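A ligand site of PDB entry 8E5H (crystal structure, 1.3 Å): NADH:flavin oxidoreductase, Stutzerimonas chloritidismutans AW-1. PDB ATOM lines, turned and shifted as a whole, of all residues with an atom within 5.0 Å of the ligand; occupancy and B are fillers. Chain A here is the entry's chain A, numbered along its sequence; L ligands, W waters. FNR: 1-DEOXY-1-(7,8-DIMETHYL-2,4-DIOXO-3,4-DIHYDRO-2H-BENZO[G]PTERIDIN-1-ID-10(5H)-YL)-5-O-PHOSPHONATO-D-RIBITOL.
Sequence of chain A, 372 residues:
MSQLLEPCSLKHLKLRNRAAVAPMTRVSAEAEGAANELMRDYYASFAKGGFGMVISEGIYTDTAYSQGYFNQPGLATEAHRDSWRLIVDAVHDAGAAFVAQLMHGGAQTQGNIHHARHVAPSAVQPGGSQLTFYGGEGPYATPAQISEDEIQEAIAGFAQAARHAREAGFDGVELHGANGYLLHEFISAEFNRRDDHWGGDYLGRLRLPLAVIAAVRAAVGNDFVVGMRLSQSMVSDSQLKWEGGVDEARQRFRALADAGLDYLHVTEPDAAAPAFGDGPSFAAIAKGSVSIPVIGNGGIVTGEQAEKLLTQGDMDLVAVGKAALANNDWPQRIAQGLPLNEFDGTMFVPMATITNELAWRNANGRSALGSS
Water W1 bridges an oxygen (O3P) of the ligand and the side-chain amino group (NZ) of Lys 322.
Water W5 lies within hydrogen-bond range of O of Ile 300 (2.7 Å), O2P of the ligand (2.8 Å) and N of Ala 323 (3.0 Å).
Water W6 lies within hydrogen-bond range of a nitrogen (N3) of the ligand (3.1 Å) and a ring nitrogen (NE2) of His 176 (3.2 Å).
Water W2 lies within hydrogen-bond range of OG1 of Thr 25 (3.0 Å) and N5 of the ligand (3.1 Å).
Residues that only touch the ligand: Tyr 134, Met 24, Ala 22, Phe 348, Val 320 and Gly 298.
Hydrophobic or aromatic side chains that line the ligand: Ala 22, Pro 23, Met 24, Tyr 134, His 176 and Phe 348.
18 residues have an atom within 4 Å of the ligand: Ala 22, Pro 23, Met 24, Thr 25, Gly 58, Gln 101, Tyr 134, His 176, Asn 179, Arg 229, Thr 267, Asn 297, Gly 298, Gly 299, Val 320, Gly 321, Lys 322 and Phe 348.
The backbone NH (N) of Ala 22 sits at hydrogen-bond distance from the backbone carbonyl oxygen (O) of Val 320 (2.9 Å).
The side-chain hydroxyl of Thr 267 sits at hydrogen-bond distance from the side-chain amide oxygen of Asn 297, at 2.6 Å.
ND2 of Asn 297 lies within hydrogen-bond range of O of Ala 319 (2.9 Å).
OD1 of Asn 297 sits at hydrogen-bond distance from NH2 of Arg 229, at 3.3 Å.
The side-chain amide oxygen (OD1) of Asn 179 sits at hydrogen-bond distance from the guanidinium group (NH1) of Arg 229, at 3.4 Å.
The side-chain amide oxygen (OE1) of Gln 101 sits close to the backbone NH (N) of Gly 58, at 3.3 Å.
The side-chain hydroxyl (OG1) of Thr 267 is in hydrogen-bond range of an oxygen (O3') of the ligand, at 3.3 Å.
An oxygen (O3') of the ligand is in hydrogen-bond range of the side-chain amide oxygen (OD1) of Asn 297 (2.5 Å).
A ring nitrogen (NE2) of His 176 lies within hydrogen-bond range of an oxygen (O2) of the ligand (3.0 Å).
N of Gly 299 lies within hydrogen-bond range of O3P of the ligand (2.9 Å).
The backbone NH of Gly 321 is in hydrogen-bond range of an oxygen (O2P) of the ligand (3.0 Å).
N of Gly 58 is in hydrogen-bond range of O4 of the ligand, 3.3 Å away.
The backbone carbonyl oxygen of Pro 23 sits at hydrogen-bond distance from an oxygen (O2') of the ligand (2.6 Å).
The guanidinium group of Arg 229 is in hydrogen-bond range of an oxygen (O2) of the ligand, at 2.7 Å.
OD1 of Asn 179 lies close to O2 of the ligand (3.3 Å).
An oxygen (O1P) of the ligand sits at hydrogen-bond distance from the backbone NH of Lys 322 (2.9 Å).
OE1 of Gln 101 lies within hydrogen-bond range of N3 of the ligand, at 2.9 Å.
The side-chain hydroxyl (OG1) of Thr 25 is in hydrogen-bond range of an oxygen (O4) of the ligand (2.5 Å).
N of Thr 25 lies close to O4 of the ligand (3.4 Å).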
ATOM      1  N   ALA A  22     -14.109  19.564  10.454  1.00  0.00           N
ATOM      2  CA  ALA A  22     -14.566  20.759  11.141  1.00  0.00           C
ATOM      3  C   ALA A  22     -15.632  20.421  12.167  1.00  0.00           C
ATOM      4  O   ALA A  22     -16.404  19.465  11.979  1.00  0.00           O
ATOM      5  CB  ALA A  22     -15.141  21.736  10.103  1.00  0.00           C
ATOM      6  N   PRO A  23     -15.723  21.220  13.237  1.00  0.00           N
ATOM      7  CA  PRO A  23     -16.761  21.004  14.262  1.00  0.00           C
ATOM      8  C   PRO A  23     -18.134  21.222  13.663  1.00  0.00           C
ATOM      9  O   PRO A  23     -18.396  22.263  13.041  1.00  0.00           O
ATOM     10  CB  PRO A  23     -16.462  22.083  15.316  1.00  0.00           C
ATOM     11  CG  PRO A  23     -15.602  23.141  14.590  1.00  0.00           C
ATOM     12  CD  PRO A  23     -14.865  22.402  13.519  1.00  0.00           C
ATOM     13  N   MET A  24     -19.051  20.273  13.880  1.00  0.00           N
ATOM     14  CA  MET A  24     -20.429  20.414  13.367  1.00  0.00           C
ATOM     15  C   MET A  24     -21.437  19.900  14.396  1.00  0.00           C
ATOM     16  O   MET A  24     -21.506  18.725  14.697  1.00  0.00           O
ATOM     17  CB  MET A  24     -20.587  19.609  12.085  1.00  0.00           C
ATOM     18  CG  MET A  24     -19.708  20.094  10.916  1.00  0.00           C
ATOM     19  SD  MET A  24     -19.858  19.116   9.420  1.00  0.00           S
ATOM     20  CE  MET A  24     -18.776  17.793   9.846  1.00  0.00           C
ATOM     21  N   THR A  25     -22.328  20.802  14.802  1.00  0.00           N
ATOM     22  CA  THR A  25     -23.397  20.534  15.759  1.00  0.00           C
ATOM     23  C   THR A  25     -24.405  19.586  15.134  1.00  0.00           C
ATOM     24  O   THR A  25     -24.911  19.855  14.033  1.00  0.00           O
ATOM     25  CB  THR A  25     -24.073  21.881  16.098  1.00  0.00           C
ATOM     26  OG1 THR A  25     -23.194  22.723  16.886  1.00  0.00           O
ATOM     27  CG2 THR A  25     -25.419  21.711  16.799  1.00  0.00           C
ATOM     28  N   ARG A  26     -24.647  18.461  15.781  1.00  0.00           N
ATOM     29  CA  ARG A  26     -25.593  17.488  15.281  1.00  0.00           C
ATOM     30  C   ARG A  26     -26.763  17.203  16.221  1.00  0.00           C
ATOM     31  O   ARG A  26     -27.630  16.424  15.858  1.00  0.00           O
ATOM     32  CB  ARG A  26     -24.884  16.162  14.984  1.00  0.00           C
ATOM     33  CG  ARG A  26     -23.684  16.262  14.026  1.00  0.00           C
ATOM     34  CD  ARG A  26     -23.943  17.008  12.705  1.00  0.00           C
ATOM     35  NE  ARG A  26     -25.025  16.387  11.938  1.00  0.00           N
ATOM     36  CZ  ARG A  26     -24.870  15.416  11.040  1.00  0.00           C
ATOM     37  NH1 ARG A  26     -23.682  14.910  10.781  1.00  0.00           N
ATOM     38  NH2 ARG A  26     -25.937  14.898  10.442  1.00  0.00           N
ATOM     39  N   GLU A  57     -18.133  18.439  17.451  1.00  0.00           N
ATOM     40  CA  GLU A  57     -19.117  19.490  17.583  1.00  0.00           C
ATOM     41  C   GLU A  57     -18.902  20.282  18.880  1.00  0.00           C
ATOM     42  O   GLU A  57     -18.255  19.825  19.839  1.00  0.00           O
ATOM     43  CB  GLU A  57     -20.532  18.883  17.676  1.00  0.00           C
ATOM     44  CG  GLU A  57     -20.765  18.002  18.856  1.00  0.00           C
ATOM     45  CD  GLU A  57     -21.839  16.987  18.611  1.00  0.00           C
ATOM     46  OE1 GLU A  57     -23.024  17.335  18.322  1.00  0.00           O
ATOM     47  OE2 GLU A  57     -21.471  15.796  18.588  1.00  0.00           O
ATOM     48  N   GLY A  58     -19.463  21.467  18.924  1.00  0.00           N
ATOM     49  CA  GLY A  58     -19.362  22.245  20.135  1.00  0.00           C
ATOM     50  C   GLY A  58     -20.030  21.588  21.324  1.00  0.00           C
ATOM     51  O   GLY A  58     -21.218  21.257  21.280  1.00  0.00           O
ATOM     52  N   GLN A 101     -14.209  20.515  21.004  1.00  0.00           N
ATOM     53  CA  GLN A 101     -14.587  21.920  20.921  1.00  0.00           C
ATOM     54  C   GLN A 101     -15.464  22.245  22.118  1.00  0.00           C
ATOM     55  O   GLN A 101     -16.434  21.532  22.388  1.00  0.00           O
ATOM     56  CB  GLN A 101     -15.318  22.251  19.628  1.00  0.00           C
ATOM     57  CG  GLN A 101     -15.505  23.796  19.548  1.00  0.00           C
ATOM     58  CD  GLN A 101     -16.279  24.255  18.364  1.00  0.00           C
ATOM     59  OE1 GLN A 101     -17.463  24.042  18.289  1.00  0.00           O
ATOM     60  NE2 GLN A 101     -15.613  24.923  17.442  1.00  0.00           N
ATOM     61  N   MET A 103     -17.857  25.125  24.007  1.00  0.00           N
ATOM     62  CA  MET A 103     -18.683  26.233  23.520  1.00  0.00           C
ATOM     63  C   MET A 103     -19.726  26.633  24.554  1.00  0.00           C
ATOM     64  O   MET A 103     -20.360  25.772  25.167  1.00  0.00           O
ATOM     65  CB  MET A 103     -19.372  25.791  22.230  1.00  0.00           C
ATOM     66  CG  MET A 103     -20.449  26.688  21.647  1.00  0.00           C
ATOM     67  SD  MET A 103     -21.083  26.237  19.973  1.00  0.00           S
ATOM     68  CE  MET A 103     -22.068  24.817  20.393  1.00  0.00           C
ATOM     69  N   PHE A 133     -32.932  23.638  12.045  1.00  0.00           N
ATOM     70  CA  PHE A 133     -32.485  22.257  12.093  1.00  0.00           C
ATOM     71  C   PHE A 133     -31.691  21.929  13.349  1.00  0.00           C
ATOM     72  O   PHE A 133     -31.257  20.776  13.483  1.00  0.00           O
ATOM     73  CB  PHE A 133     -31.768  21.782  10.819  1.00  0.00           C
ATOM     74  CG  PHE A 133     -30.628  22.614  10.379  1.00  0.00           C
ATOM     75  CD1 PHE A 133     -29.626  22.968  11.238  1.00  0.00           C
ATOM     76  CD2 PHE A 133     -30.471  22.901   9.028  1.00  0.00           C
ATOM     77  CE1 PHE A 133     -28.545  23.733  10.807  1.00  0.00           C
ATOM     78  CE2 PHE A 133     -29.402  23.632   8.575  1.00  0.00           C
ATOM     79  CZ  PHE A 133     -28.421  24.038   9.469  1.00  0.00           C
ATOM     80  N   TYR A 134     -31.520  22.874  14.291  1.00  0.00           N
ATOM     81  CA  TYR A 134     -31.076  22.548  15.642  1.00  0.00           C
ATOM     82  C   TYR A 134     -32.184  22.575  16.688  1.00  0.00           C
ATOM     83  O   TYR A 134     -31.907  22.297  17.863  1.00  0.00           O
ATOM     84  CB  TYR A 134     -29.969  23.502  16.153  1.00  0.00           C
ATOM     85  CG  TYR A 134     -28.760  23.603  15.301  1.00  0.00           C
ATOM     86  CD1 TYR A 134     -28.321  22.520  14.531  1.00  0.00           C
ATOM     87  CD2 TYR A 134     -28.004  24.765  15.288  1.00  0.00           C
ATOM     88  CE1 TYR A 134     -27.214  22.625  13.733  1.00  0.00           C
ATOM     89  CE2 TYR A 134     -26.875  24.868  14.490  1.00  0.00           C
ATOM     90  CZ  TYR A 134     -26.485  23.786  13.704  1.00  0.00           C
ATOM     91  OH  TYR A 134     -25.375  23.766  12.862  1.00  0.00           O
ATOM     92  N   HIS A 176     -14.236  27.801  21.751  1.00  0.00           N
ATOM     93  CA  HIS A 176     -15.051  28.355  20.674  1.00  0.00           C
ATOM     94  C   HIS A 176     -15.160  29.855  20.845  1.00  0.00           C
ATOM     95  O   HIS A 176     -16.049  30.354  21.552  1.00  0.00           O
ATOM     96  CB  HIS A 176     -16.422  27.700  20.634  1.00  0.00           C
ATOM     97  CG  HIS A 176     -17.125  27.878  19.349  1.00  0.00           C
ATOM     98  ND1 HIS A 176     -16.779  28.865  18.449  1.00  0.00           N
ATOM     99  CD2 HIS A 176     -18.136  27.173  18.798  1.00  0.00           C
ATOM    100  CE1 HIS A 176     -17.575  28.750  17.397  1.00  0.00           C
ATOM    101  NE2 HIS A 176     -18.395  27.741  17.582  1.00  0.00           N
ATOM    102  N   ASN A 179     -18.253  32.344  15.539  1.00  0.00           N
ATOM    103  CA  ASN A 179     -19.588  32.066  15.045  1.00  0.00           C
ATOM    104  C   ASN A 179     -20.704  32.694  15.866  1.00  0.00           C
ATOM    105  O   ASN A 179     -21.860  32.281  15.715  1.00  0.00           O
ATOM    106  CB  ASN A 179     -19.799  30.560  14.870  1.00  0.00           C
ATOM    107  CG  ASN A 179     -18.807  29.955  13.936  1.00  0.00           C
ATOM    108  OD1 ASN A 179     -18.044  29.026  14.306  1.00  0.00           O
ATOM    109  ND2 ASN A 179     -18.728  30.480  12.750  1.00  0.00           N
ATOM    110  N   ARG A 229     -10.960  28.779  18.162  1.00  0.00           N
ATOM    111  CA  ARG A 229     -11.603  29.093  16.888  1.00  0.00           C
ATOM    112  C   ARG A 229     -12.038  30.556  16.898  1.00  0.00           C
ATOM    113  O   ARG A 229     -12.588  31.067  17.900  1.00  0.00           O
ATOM    114  CB  ARG A 229     -12.819  28.204  16.643  1.00  0.00           C
ATOM    115  CG  ARG A 229     -13.188  28.132  15.176  1.00  0.00           C
ATOM    116  CD  ARG A 229     -14.307  27.178  14.821  1.00  0.00           C
ATOM    117  NE  ARG A 229     -14.131  26.739  13.431  1.00  0.00           N
ATOM    118  CZ  ARG A 229     -15.088  26.274  12.648  1.00  0.00           C
ATOM    119  NH1 ARG A 229     -16.348  26.426  12.949  1.00  0.00           N
ATOM    120  NH2 ARG A 229     -14.747  25.685  11.524  1.00  0.00           N
ATOM    121  N   THR A 267     -12.367  30.589  10.596  1.00  0.00           N
ATOM    122  CA  THR A 267     -13.449  30.208   9.691  1.00  0.00           C
ATOM    123  C   THR A 267     -14.080  31.457   9.097  1.00  0.00           C
ATOM    124  O   THR A 267     -14.238  32.463   9.797  1.00  0.00           O
ATOM    125  CB  THR A 267     -14.478  29.335  10.415  1.00  0.00           C
ATOM    126  OG1 THR A 267     -15.516  28.992   9.516  1.00  0.00           O
ATOM    127  CG2 THR A 267     -15.108  30.003  11.605  1.00  0.00           C
ATOM    128  N   ASN A 297     -10.754  27.276   7.243  1.00  0.00           N
ATOM    129  CA  ASN A 297     -12.051  26.665   7.016  1.00  0.00           C
ATOM    130  C   ASN A 297     -12.965  27.638   6.302  1.00  0.00           C
ATOM    131  O   ASN A 297     -12.957  28.852   6.571  1.00  0.00           O
ATOM    132  CB  ASN A 297     -12.706  26.276   8.338  1.00  0.00           C
ATOM    133  CG  ASN A 297     -14.139  25.870   8.151  1.00  0.00           C
ATOM    134  OD1 ASN A 297     -15.057  26.671   8.343  1.00  0.00           O
ATOM    135  ND2 ASN A 297     -14.353  24.613   7.802  1.00  0.00           N
ATOM    136  N   GLY A 298     -13.814  27.081   5.440  1.00  0.00           N
ATOM    137  CA  GLY A 298     -14.947  27.774   4.866  1.00  0.00           C
ATOM    138  C   GLY A 298     -15.059  27.503   3.372  1.00  0.00           C
ATOM    139  O   GLY A 298     -14.384  28.153   2.571  1.00  0.00           O
ATOM    140  N   GLY A 299     -15.930  26.559   2.980  1.00  0.00           N
ATOM    141  CA  GLY A 299     -16.185  26.340   1.562  1.00  0.00           C
ATOM    142  C   GLY A 299     -15.127  25.546   0.830  1.00  0.00           C
ATOM    143  O   GLY A 299     -15.078  25.579  -0.403  1.00  0.00           O
ATOM    144  N   ILE A 300     -14.262  24.849   1.543  1.00  0.00           N
ATOM    145  CA  ILE A 300     -13.217  24.058   0.918  1.00  0.00           C
ATOM    146  C   ILE A 300     -13.825  22.688   0.609  1.00  0.00           C
ATOM    147  O   ILE A 300     -14.122  21.924   1.529  1.00  0.00           O
ATOM    148  CB  ILE A 300     -11.972  23.950   1.805  1.00  0.00           C
ATOM    149  CG1 ILE A 300     -11.461  25.331   2.238  1.00  0.00           C
ATOM    150  CG2 ILE A 300     -10.884  23.134   1.068  1.00  0.00           C
ATOM    151  CD1 ILE A 300     -10.452  25.285   3.415  1.00  0.00           C
ATOM    152  N   ALA A 319      -9.643  22.371   7.545  1.00  0.00           N
ATOM    153  CA  ALA A 319     -10.809  21.761   8.173  1.00  0.00           C
ATOM    154  C   ALA A 319     -11.972  21.827   7.202  1.00  0.00           C
ATOM    155  O   ALA A 319     -12.289  22.902   6.676  1.00  0.00           O
ATOM    156  CB  ALA A 319     -11.141  22.440   9.494  1.00  0.00           C
ATOM    157  N   VAL A 320     -12.619  20.692   6.992  1.00  0.00           N
ATOM    158  CA  VAL A 320     -13.788  20.618   6.140  1.00  0.00           C
ATOM    159  C   VAL A 320     -14.972  20.056   6.917  1.00  0.00           C
ATOM    160  O   VAL A 320     -14.844  19.111   7.705  1.00  0.00           O
ATOM    161  CB  VAL A 320     -13.564  19.820   4.849  1.00  0.00           C
ATOM    162  CG1 VAL A 320     -12.602  20.534   3.986  1.00  0.00           C
ATOM    163  CG2 VAL A 320     -13.108  18.474   5.157  1.00  0.00           C
ATOM    164  N   GLY A 321     -16.121  20.693   6.696  1.00  0.00           N
ATOM    165  CA  GLY A 321     -17.356  20.277   7.310  1.00  0.00           C
ATOM    166  C   GLY A 321     -18.231  19.571   6.301  1.00  0.00           C
ATOM    167  O   GLY A 321     -18.315  18.344   6.269  1.00  0.00           O
ATOM    168  N   LYS A 322     -18.878  20.358   5.446  1.00  0.00           N
ATOM    169  CA  LYS A 322     -19.749  19.758   4.450  1.00  0.00           C
ATOM    170  C   LYS A 322     -19.068  18.682   3.627  1.00  0.00           C
ATOM    171  O   LYS A 322     -19.677  17.638   3.343  1.00  0.00           O
ATOM    172  CB  LYS A 322     -20.358  20.857   3.574  1.00  0.00           C
ATOM    173  CG  LYS A 322     -21.383  21.683   4.304  1.00  0.00           C
ATOM    174  CD  LYS A 322     -21.887  22.862   3.452  1.00  0.00           C
ATOM    175  CE  LYS A 322     -21.542  24.212   4.059  1.00  0.00           C
ATOM    176  NZ  LYS A 322     -22.313  25.300   3.383  1.00  0.00           N
ATOM    177  N   ALA A 323     -17.836  18.924   3.179  1.00  0.00           N
ATOM    178  CA  ALA A 323     -17.159  17.904   2.379  1.00  0.00           C
ATOM    179  C   ALA A 323     -16.938  16.611   3.147  1.00  0.00           C
ATOM    180  O   ALA A 323     -16.893  15.530   2.545  1.00  0.00           O
ATOM    181  CB  ALA A 323     -15.821  18.413   1.831  1.00  0.00           C
ATOM    182  N   PHE A 348     -30.053  17.304   6.295  1.00  0.00           N
ATOM    183  CA  PHE A 348     -30.314  17.921   7.592  1.00  0.00           C
ATOM    184  C   PHE A 348     -31.788  18.212   7.856  1.00  0.00           C
ATOM    185  O   PHE A 348     -32.106  18.751   8.920  1.00  0.00           O
ATOM    186  CB  PHE A 348     -29.573  19.266   7.818  1.00  0.00           C
ATOM    187  CG  PHE A 348     -28.089  19.217   7.697  1.00  0.00           C
ATOM    188  CD1 PHE A 348     -27.347  18.168   8.237  1.00  0.00           C
ATOM    189  CD2 PHE A 348     -27.412  20.315   7.207  1.00  0.00           C
ATOM    190  CE1 PHE A 348     -25.970  18.178   8.193  1.00  0.00           C
ATOM    191  CE2 PHE A 348     -26.030  20.330   7.131  1.00  0.00           C
ATOM    192  CZ  PHE A 348     -25.307  19.279   7.634  1.00  0.00           C
ATOM    193  N   ALA A 352     -30.860  18.315  12.021  1.00  0.00           N
ATOM    194  CA  ALA A 352     -29.545  17.857  11.561  1.00  0.00           C
ATOM    195  C   ALA A 352     -28.980  16.703  12.397  1.00  0.00           C
ATOM    196  O   ALA A 352     -27.766  16.669  12.662  1.00  0.00           O
ATOM    197  CB  ALA A 352     -28.600  19.069  11.595  1.00  0.00           C
HETATM  198  C9A FNR L   1     -21.413  23.814  11.650  1.00  0.00           C
HETATM  199  N10 FNR L   1     -20.372  24.695  12.051  1.00  0.00           N
HETATM  200  CAA FNR L   1     -19.961  24.734  13.377  1.00  0.00           C
HETATM  201  N1  FNR L   1     -18.813  25.380  13.757  1.00  0.00           N
HETATM  202  C2  FNR L   1     -18.355  25.333  15.045  1.00  0.00           C
HETATM  203  O2  FNR L   1     -17.389  25.950  15.379  1.00  0.00           O
HETATM  204  N3  FNR L   1     -19.057  24.607  15.956  1.00  0.00           N
HETATM  205  C4  FNR L   1     -20.209  23.912  15.651  1.00  0.00           C
HETATM  206  O4  FNR L   1     -20.752  23.271  16.546  1.00  0.00           O
HETATM  207  C4A FNR L   1     -20.652  23.980  14.319  1.00  0.00           C
HETATM  208  N5  FNR L   1     -21.801  23.437  13.937  1.00  0.00           N
HETATM  209  C5A FNR L   1     -22.131  23.177  12.632  1.00  0.00           C
HETATM  210  C6  FNR L   1     -23.129  22.270  12.319  1.00  0.00           C
HETATM  211  C7  FNR L   1     -23.433  21.993  11.021  1.00  0.00           C
HETATM  212  C7M FNR L   1     -24.535  21.014  10.714  1.00  0.00           C
HETATM  213  C8  FNR L   1     -22.688  22.635   9.983  1.00  0.00           C
HETATM  214  C8M FNR L   1     -22.990  22.342   8.541  1.00  0.00           C
HETATM  215  C9  FNR L   1     -21.683  23.520  10.315  1.00  0.00           C
HETATM  216  C1' FNR L   1     -19.560  25.342  10.992  1.00  0.00           C
HETATM  217  C2' FNR L   1     -18.565  24.359  10.398  1.00  0.00           C
HETATM  218  O2' FNR L   1     -17.544  24.033  11.327  1.00  0.00           O
HETATM  219  C3' FNR L   1     -17.879  24.961   9.182  1.00  0.00           C
HETATM  220  O3' FNR L   1     -17.138  26.070   9.648  1.00  0.00           O
HETATM  221  C4' FNR L   1     -18.860  25.459   8.131  1.00  0.00           C
HETATM  222  O4' FNR L   1     -19.755  24.393   7.782  1.00  0.00           O
HETATM  223  C5' FNR L   1     -18.162  25.994   6.891  1.00  0.00           C
HETATM  224  O5' FNR L   1     -17.115  25.090   6.464  1.00  0.00           O
HETATM  225  P   FNR L   1     -17.468  24.003   5.323  1.00  0.00           P
HETATM  226  O1P FNR L   1     -18.616  23.229   5.873  1.00  0.00           O
HETATM  227  O2P FNR L   1     -16.213  23.215   5.098  1.00  0.00           O
HETATM  228  O3P FNR L   1     -17.900  24.761   4.118  1.00  0.00           O
HETATM  229  O   HOH W   1     -19.719  26.496   3.360  1.00  0.00           O
HETATM  230  O   HOH W   2     -22.990  25.537  15.875  1.00  0.00           O
HETATM  231  O   HOH W   3     -18.124  23.489   1.716  1.00  0.00           O
HETATM  232  O   HOH W   4     -18.146  29.072   6.255  1.00  0.00           O
HETATM  233  O   HOH W   5     -16.385  21.510   2.939  1.00  0.00           O
HETATM  234  O   HOH W   6     -20.788  27.092  15.525  1.00  0.00           O
HETATM  235  O   HOH W   7     -22.165  25.679   7.116  1.00  0.00           O
HETATM  236  O   HOH W   8     -21.475  27.679  12.937  1.00  0.00           O
HETATM  237  O   HOH W   9     -13.895  24.315   4.605  1.00  0.00           O
